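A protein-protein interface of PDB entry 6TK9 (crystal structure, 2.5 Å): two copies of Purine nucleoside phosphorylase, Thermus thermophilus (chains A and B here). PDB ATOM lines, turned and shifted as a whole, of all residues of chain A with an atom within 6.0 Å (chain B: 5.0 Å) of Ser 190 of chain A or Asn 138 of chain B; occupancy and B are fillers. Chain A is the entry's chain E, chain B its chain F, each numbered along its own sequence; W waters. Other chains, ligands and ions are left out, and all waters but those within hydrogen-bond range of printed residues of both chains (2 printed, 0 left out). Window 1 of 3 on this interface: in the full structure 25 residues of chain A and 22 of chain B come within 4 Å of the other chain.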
ATOM      1  N   PHE A 186      17.045 -12.356   5.923  1.00  0.00           N
ATOM      2  CA  PHE A 186      18.060 -13.433   6.034  1.00  0.00           C
ATOM      3  C   PHE A 186      19.391 -12.747   6.345  1.00  0.00           C
ATOM      4  O   PHE A 186      19.717 -11.753   5.655  1.00  0.00           O
ATOM      5  CB  PHE A 186      18.098 -14.219   4.723  1.00  0.00           C
ATOM      6  CG  PHE A 186      19.136 -15.303   4.609  1.00  0.00           C
ATOM      7  CD1 PHE A 186      18.900 -16.567   5.116  1.00  0.00           C
ATOM      8  CD2 PHE A 186      20.301 -15.100   3.885  1.00  0.00           C
ATOM      9  CE1 PHE A 186      19.837 -17.583   4.970  1.00  0.00           C
ATOM     10  CE2 PHE A 186      21.238 -16.115   3.735  1.00  0.00           C
ATOM     11  CZ  PHE A 186      21.005 -17.357   4.282  1.00  0.00           C
ATOM     12  N   MET A 187      20.122 -13.214   7.358  1.00  0.00           N
ATOM     13  CA  MET A 187      21.259 -12.448   7.924  1.00  0.00           C
ATOM     14  C   MET A 187      22.361 -12.246   6.875  1.00  0.00           C
ATOM     15  O   MET A 187      22.870 -11.108   6.762  1.00  0.00           O
ATOM     16  CB  MET A 187      21.832 -13.123   9.164  1.00  0.00           C
ATOM     17  CG  MET A 187      22.398 -14.502   8.942  1.00  0.00           C
ATOM     18  SD  MET A 187      22.713 -15.225  10.557  1.00  0.00           S
ATOM     19  CE  MET A 187      24.148 -14.250  11.012  1.00  0.00           C
ATOM     20  N   GLY A 188      22.699 -13.277   6.110  1.00  0.00           N
ATOM     21  CA  GLY A 188      23.794 -13.196   5.128  1.00  0.00           C
ATOM     22  C   GLY A 188      25.133 -13.187   5.849  1.00  0.00           C
ATOM     23  O   GLY A 188      25.163 -13.486   7.044  1.00  0.00           O
ATOM     24  N   PRO A 189      26.255 -12.796   5.193  1.00  0.00           N
ATOM     25  CA  PRO A 189      26.247 -12.252   3.840  1.00  0.00           C
ATOM     26  C   PRO A 189      26.286 -13.316   2.743  1.00  0.00           C
ATOM     27  O   PRO A 189      26.171 -12.950   1.594  1.00  0.00           O
ATOM     28  CB  PRO A 189      27.591 -11.512   3.792  1.00  0.00           C
ATOM     29  CG  PRO A 189      28.497 -12.459   4.544  1.00  0.00           C
ATOM     30  CD  PRO A 189      27.630 -12.887   5.714  1.00  0.00           C
ATOM     31  N   SER A 190      26.585 -14.573   3.081  1.00  0.00           N
ATOM     32  CA  SER A 190      26.448 -15.669   2.093  1.00  0.00           C
ATOM     33  C   SER A 190      24.999 -15.630   1.612  1.00  0.00           C
ATOM     34  O   SER A 190      24.119 -15.234   2.394  1.00  0.00           O
ATOM     35  CB  SER A 190      26.829 -17.023   2.647  1.00  0.00           C
ATOM     36  OG  SER A 190      26.003 -17.390   3.738  1.00  0.00           O
ATOM     37  N   PHE A 191      24.771 -15.929   0.347  1.00  0.00           N
ATOM     38  CA  PHE A 191      23.415 -16.180  -0.185  1.00  0.00           C
ATOM     39  C   PHE A 191      22.901 -17.495   0.404  1.00  0.00           C
ATOM     40  O   PHE A 191      23.700 -18.328   0.919  1.00  0.00           O
ATOM     41  CB  PHE A 191      23.432 -16.212  -1.713  1.00  0.00           C
ATOM     42  CG  PHE A 191      23.522 -14.852  -2.352  1.00  0.00           C
ATOM     43  CD1 PHE A 191      22.623 -13.851  -2.010  1.00  0.00           C
ATOM     44  CD2 PHE A 191      24.486 -14.577  -3.312  1.00  0.00           C
ATOM     45  CE1 PHE A 191      22.692 -12.608  -2.609  1.00  0.00           C
ATOM     46  CE2 PHE A 191      24.551 -13.330  -3.916  1.00  0.00           C
ATOM     47  CZ  PHE A 191      23.665 -12.346  -3.550  1.00  0.00           C
ATOM     48  N   ALA A 192      21.589 -17.687   0.305  1.00  0.00           N
ATOM     49  CA  ALA A 192      20.873 -18.836   0.889  1.00  0.00           C
ATOM     50  C   ALA A 192      21.147 -20.088   0.039  1.00  0.00           C
ATOM     51  O   ALA A 192      21.377 -19.960  -1.189  1.00  0.00           O
ATOM     52  CB  ALA A 192      19.405 -18.490   0.987  1.00  0.00           C
ATOM     53  N   MET A 210      18.760  -8.885   2.875  1.00  0.00           N
ATOM     54  CA  MET A 210      19.661  -8.873   4.056  1.00  0.00           C
ATOM     55  C   MET A 210      19.514  -7.557   4.834  1.00  0.00           C
ATOM     56  O   MET A 210      20.453  -7.241   5.600  1.00  0.00           O
ATOM     57  CB  MET A 210      21.104  -9.097   3.599  1.00  0.00           C
ATOM     58  CG  MET A 210      21.267 -10.425   2.881  1.00  0.00           C
ATOM     59  SD  MET A 210      22.915 -10.659   2.206  1.00  0.00           S
ATOM     60  CE  MET A 210      22.663 -12.127   1.220  1.00  0.00           C
ATOM     61  N   ALA B  89      31.252 -18.254  14.996  1.00  0.00           N
ATOM     62  CA  ALA B  89      31.217 -18.851  13.643  1.00  0.00           C
ATOM     63  C   ALA B  89      32.596 -18.723  12.979  1.00  0.00           C
ATOM     64  O   ALA B  89      33.114 -19.766  12.521  1.00  0.00           O
ATOM     65  CB  ALA B  89      30.155 -18.175  12.817  1.00  0.00           C
ATOM     66  N   TYR B 131      22.207 -28.017   2.882  1.00  0.00           N
ATOM     67  CA  TYR B 131      22.208 -27.688   4.321  1.00  0.00           C
ATOM     68  C   TYR B 131      21.172 -26.601   4.602  1.00  0.00           C
ATOM     69  O   TYR B 131      20.729 -25.894   3.678  1.00  0.00           O
ATOM     70  CB  TYR B 131      23.581 -27.179   4.756  1.00  0.00           C
ATOM     71  CG  TYR B 131      23.925 -25.817   4.213  1.00  0.00           C
ATOM     72  CD1 TYR B 131      23.505 -24.666   4.857  1.00  0.00           C
ATOM     73  CD2 TYR B 131      24.695 -25.679   3.069  1.00  0.00           C
ATOM     74  CE1 TYR B 131      23.819 -23.409   4.362  1.00  0.00           C
ATOM     75  CE2 TYR B 131      25.010 -24.429   2.555  1.00  0.00           C
ATOM     76  CZ  TYR B 131      24.573 -23.292   3.207  1.00  0.00           C
ATOM     77  OH  TYR B 131      24.859 -22.063   2.697  1.00  0.00           O
ATOM     78  N   ASN B 133      20.926 -23.581   7.733  1.00  0.00           N
ATOM     79  CA  ASN B 133      21.476 -22.902   8.936  1.00  0.00           C
ATOM     80  C   ASN B 133      20.304 -22.550   9.855  1.00  0.00           C
ATOM     81  O   ASN B 133      19.493 -21.702   9.456  1.00  0.00           O
ATOM     82  CB  ASN B 133      22.313 -21.679   8.544  1.00  0.00           C
ATOM     83  CG  ASN B 133      23.043 -21.025   9.695  1.00  0.00           C
ATOM     84  OD1 ASN B 133      23.895 -20.170   9.485  1.00  0.00           O
ATOM     85  ND2 ASN B 133      22.696 -21.375  10.915  1.00  0.00           N
ATOM     86  N   GLY B 136      21.764 -19.486  13.660  1.00  0.00           N
ATOM     87  CA  GLY B 136      21.591 -18.029  13.795  1.00  0.00           C
ATOM     88  C   GLY B 136      22.927 -17.321  13.813  1.00  0.00           C
ATOM     89  O   GLY B 136      23.017 -16.301  14.515  1.00  0.00           O
ATOM     90  N   ALA B 137      23.919 -17.865  13.090  1.00  0.00           N
ATOM     91  CA  ALA B 137      25.294 -17.321  12.957  1.00  0.00           C
ATOM     92  C   ALA B 137      25.918 -17.700  11.607  1.00  0.00           C
ATOM     93  O   ALA B 137      25.745 -18.834  11.140  1.00  0.00           O
ATOM     94  CB  ALA B 137      26.159 -17.809  14.088  1.00  0.00           C
ATOM     95  N   ASN B 138      26.664 -16.771  11.019  1.00  0.00           N
ATOM     96  CA  ASN B 138      27.296 -16.923   9.685  1.00  0.00           C
ATOM     97  C   ASN B 138      28.780 -16.616   9.836  1.00  0.00           C
ATOM     98  O   ASN B 138      29.142 -15.592  10.398  1.00  0.00           O
ATOM     99  CB  ASN B 138      26.608 -16.023   8.660  1.00  0.00           C
ATOM    100  CG  ASN B 138      26.923 -16.409   7.231  1.00  0.00           C
ATOM    101  OD1 ASN B 138      28.053 -16.238   6.762  1.00  0.00           O
ATOM    102  ND2 ASN B 138      25.914 -16.895   6.525  1.00  0.00           N
ATOM    103  N   PRO B 139      29.684 -17.492   9.363  1.00  0.00           N
ATOM    104  CA  PRO B 139      31.120 -17.244   9.492  1.00  0.00           C
ATOM    105  C   PRO B 139      31.646 -15.999   8.766  1.00  0.00           C
ATOM    106  O   PRO B 139      32.726 -15.581   9.088  1.00  0.00           O
ATOM    107  CB  PRO B 139      31.786 -18.478   8.864  1.00  0.00           C
ATOM    108  CG  PRO B 139      30.693 -19.138   8.044  1.00  0.00           C
ATOM    109  CD  PRO B 139      29.381 -18.771   8.707  1.00  0.00           C
ATOM    110  N   LEU B 140      30.918 -15.475   7.780  1.00  0.00           N
ATOM    111  CA  LEU B 140      31.391 -14.372   6.897  1.00  0.00           C
ATOM    112  C   LEU B 140      30.887 -13.026   7.425  1.00  0.00           C
ATOM    113  O   LEU B 140      31.184 -12.014   6.813  1.00  0.00           O
ATOM    114  CB  LEU B 140      30.869 -14.613   5.478  1.00  0.00           C
ATOM    115  CG  LEU B 140      31.296 -15.915   4.814  1.00  0.00           C
ATOM    116  CD1 LEU B 140      30.699 -16.031   3.426  1.00  0.00           C
ATOM    117  CD2 LEU B 140      32.807 -15.996   4.734  1.00  0.00           C
ATOM    118  N   ARG B 141      30.086 -13.022   8.483  1.00  0.00           N
ATOM    119  CA  ARG B 141      29.653 -11.769   9.143  1.00  0.00           C
ATOM    120  C   ARG B 141      30.899 -10.952   9.501  1.00  0.00           C
ATOM    121  O   ARG B 141      31.751 -11.462  10.243  1.00  0.00           O
ATOM    122  CB  ARG B 141      28.825 -12.041  10.401  1.00  0.00           C
ATOM    123  CG  ARG B 141      28.380 -10.766  11.101  1.00  0.00           C
ATOM    124  CD  ARG B 141      27.064 -10.953  11.806  1.00  0.00           C
ATOM    125  NE  ARG B 141      26.606  -9.675  12.306  1.00  0.00           N
ATOM    126  CZ  ARG B 141      26.928  -9.163  13.486  1.00  0.00           C
ATOM    127  NH1 ARG B 141      27.706  -9.839  14.315  1.00  0.00           N
ATOM    128  NH2 ARG B 141      26.442  -7.987  13.847  1.00  0.00           N
ATOM    129  N   ARG B 151      32.056 -10.782  -1.303  1.00  0.00           N
ATOM    130  CA  ARG B 151      31.161 -10.313  -0.220  1.00  0.00           C
ATOM    131  C   ARG B 151      29.949 -11.262  -0.088  1.00  0.00           C
ATOM    132  O   ARG B 151      29.622 -11.615   1.065  1.00  0.00           O
ATOM    133  CB  ARG B 151      30.725  -8.870  -0.503  1.00  0.00           C
ATOM    134  CG  ARG B 151      29.632  -8.344   0.423  1.00  0.00           C
ATOM    135  CD  ARG B 151      30.118  -7.954   1.816  1.00  0.00           C
ATOM    136  NE  ARG B 151      30.432  -9.095   2.652  1.00  0.00           N
ATOM    137  CZ  ARG B 151      30.834  -9.018   3.914  1.00  0.00           C
ATOM    138  NH1 ARG B 151      30.984  -7.833   4.493  1.00  0.00           N
ATOM    139  NH2 ARG B 151      31.090 -10.130   4.590  1.00  0.00           N
ATOM    140  N   PHE B 152      29.315 -11.653  -1.208  1.00  0.00           N
ATOM    141  CA  PHE B 152      28.051 -12.441  -1.233  1.00  0.00           C
ATOM    142  C   PHE B 152      28.212 -13.761  -2.007  1.00  0.00           C
ATOM    143  O   PHE B 152      27.633 -13.955  -3.082  1.00  0.00           O
ATOM    144  CB  PHE B 152      26.931 -11.596  -1.841  1.00  0.00           C
ATOM    145  CG  PHE B 152      26.718 -10.234  -1.232  1.00  0.00           C
ATOM    146  CD1 PHE B 152      26.150 -10.090   0.018  1.00  0.00           C
ATOM    147  CD2 PHE B 152      27.013  -9.085  -1.952  1.00  0.00           C
ATOM    148  CE1 PHE B 152      25.923  -8.830   0.557  1.00  0.00           C
ATOM    149  CE2 PHE B 152      26.770  -7.828  -1.424  1.00  0.00           C
ATOM    150  CZ  PHE B 152      26.227  -7.700  -0.166  1.00  0.00           C
ATOM    151  N   PRO B 153      28.938 -14.763  -1.464  1.00  0.00           N
ATOM    152  CA  PRO B 153      29.180 -16.002  -2.198  1.00  0.00           C
ATOM    153  C   PRO B 153      27.881 -16.769  -2.425  1.00  0.00           C
ATOM    154  O   PRO B 153      27.141 -16.928  -1.509  1.00  0.00           O
ATOM    155  CB  PRO B 153      30.111 -16.812  -1.302  1.00  0.00           C
ATOM    156  CG  PRO B 153      29.846 -16.262   0.080  1.00  0.00           C
ATOM    157  CD  PRO B 153      29.506 -14.797  -0.113  1.00  0.00           C
ATOM    158  N   MET B 155      25.653 -19.966  -2.785  1.00  0.00           N
ATOM    159  CA  MET B 155      25.656 -21.217  -1.971  1.00  0.00           C
ATOM    160  C   MET B 155      24.858 -22.322  -2.671  1.00  0.00           C
ATOM    161  O   MET B 155      24.669 -23.389  -2.072  1.00  0.00           O
ATOM    162  CB  MET B 155      25.075 -20.970  -0.577  1.00  0.00           C
ATOM    163  CG  MET B 155      25.986 -20.111   0.293  1.00  0.00           C
ATOM    164  SD  MET B 155      27.713 -20.693   0.279  1.00  0.00           S
ATOM    165  CE  MET B 155      27.496 -22.244   1.145  1.00  0.00           C
ATOM    166  N   ILE B 217      30.046 -22.984   4.292  1.00  0.00           N
ATOM    167  CA  ILE B 217      29.961 -21.570   3.827  1.00  0.00           C
ATOM    168  C   ILE B 217      31.386 -21.040   3.611  1.00  0.00           C
ATOM    169  O   ILE B 217      31.642 -20.524   2.507  1.00  0.00           O
ATOM    170  CB  ILE B 217      29.121 -20.743   4.814  1.00  0.00           C
ATOM    171  CG1 ILE B 217      27.645 -21.159   4.755  1.00  0.00           C
ATOM    172  CG2 ILE B 217      29.285 -19.253   4.576  1.00  0.00           C
ATOM    173  CD1 ILE B 217      26.901 -21.029   6.073  1.00  0.00           C
HETATM  174  O   HOH W   1      22.779 -19.025  -3.255  1.00  0.00           O
HETATM  175  O   HOH W   2      23.561 -19.875   3.332  1.00  0.00           O
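The backbone NH (N) of Phe 191 of chain A is in hydrogen-bond range of the backbone carbonyl oxygen (O) of Pro 153 of chain B (3.2 Å).
The side-chain amide nitrogen (ND2) of Asn 138 of chain B is in hydrogen-bond range of the side-chain hydroxyl (OG) of Ser 190 of chain A (2.8 Å).
The side-chain amide oxygen (OD1) of Asn 133 of chain B sits close to the backbone carbonyl oxygen (O) of Ala 137 of chain B (2.8 Å).
OD1 of Asn 138 of chain B is in hydrogen-bond range of N of Leu 140 of chain B (3.1 Å).
The backbone NH (N) of Gly 136 of chain B sits close to the side-chain amide nitrogen (ND2) of Asn 133 of chain B (3.5 Å).
The backbone carbonyl oxygen (O) of Leu 140 of chain B sits at hydrogen-bond distance from the guanidinium group (NH2) of Arg 151 of chain B.
Gly 136 of chain B touches Met 187 of chain A.
Ala 137 of chain B touches Met 187 of chain A (CA to CE, 3.8 Å).
Met 187 of chain A touches Asn 138 of chain B (CE to N, 3.6 Å).
O of Gly 188 of chain A touches CB of Asn 138 of chain B, at 3.3 Å.
Arg 141 of chain B touches Pro 189 of chain A.
Phe 152 of chain B touches Pro 189 of chain A.
Ser 190 of chain A touches Pro 153 of chain B (CA to CD, 3.9 Å).
CB of Ser 190 of chain A touches CG of Met 155 of chain B, at 3.97 Å.
Ala 192 of chain A touches Met 155 of chain B.
Met 210 of chain A touches Phe 152 of chain B.
Asn 138 of chain B touches just these residues of chain A: Met 187 (3.6 Å), Gly 188 (3.3 Å), Pro 189 (3.5 Å) and Ser 190 (2.8 Å).
Of the printed residues of chain B, Pro 189 of chain A touches Asn 138, Leu 140, Arg 141, Arg 151 and Phe 152.
Printed residues of chain B within 4 Å of Gly 188 of chain A: Asn 138.
Tyr 131 of chain B touches none of the printed residues of chain A.
Ala 89 of chain B touches none of the printed residues of chain A.
The nearest residue of chain A that does not touch Asn 138 of chain B is Phe 186 of chain A (5.4 Å).
The nearest printed residue of chain B that does not touch Pro 189 of chain A is Pro 153 of chain B (4.2 Å).
Of the 8 printed residues of chain A, 7 touch a printed residue of chain B.
Printed residues of chain A that touch a printed residue of chain B: Met 187, Gly 188, Pro 189, Ser 190, Phe 191, Ala 192 and Met 210.
Hydrophobic or aromatic side chains of chain A that line the printed part of chain B: Met 187, Pro 189, Phe 191 and Met 210.
Among the printed residues, no Asp or Glu carboxylate lies within 4 Å of a Lys or Arg side-chain nitrogen of the other chain.
No position is printed for both chains.
Water W2 bridges the side-chain hydroxyl of Tyr 131 of chain B (2.6 Å) and the backbone carbonyl oxygen of Phe 191 of chain A (2.9 Å).
Water W1 bridges the backbone carbonyl oxygen (O) of Ala 192 of chain A (2.7 Å) and the backbone NH (N) of Met 155 of chain B (3.1 Å).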
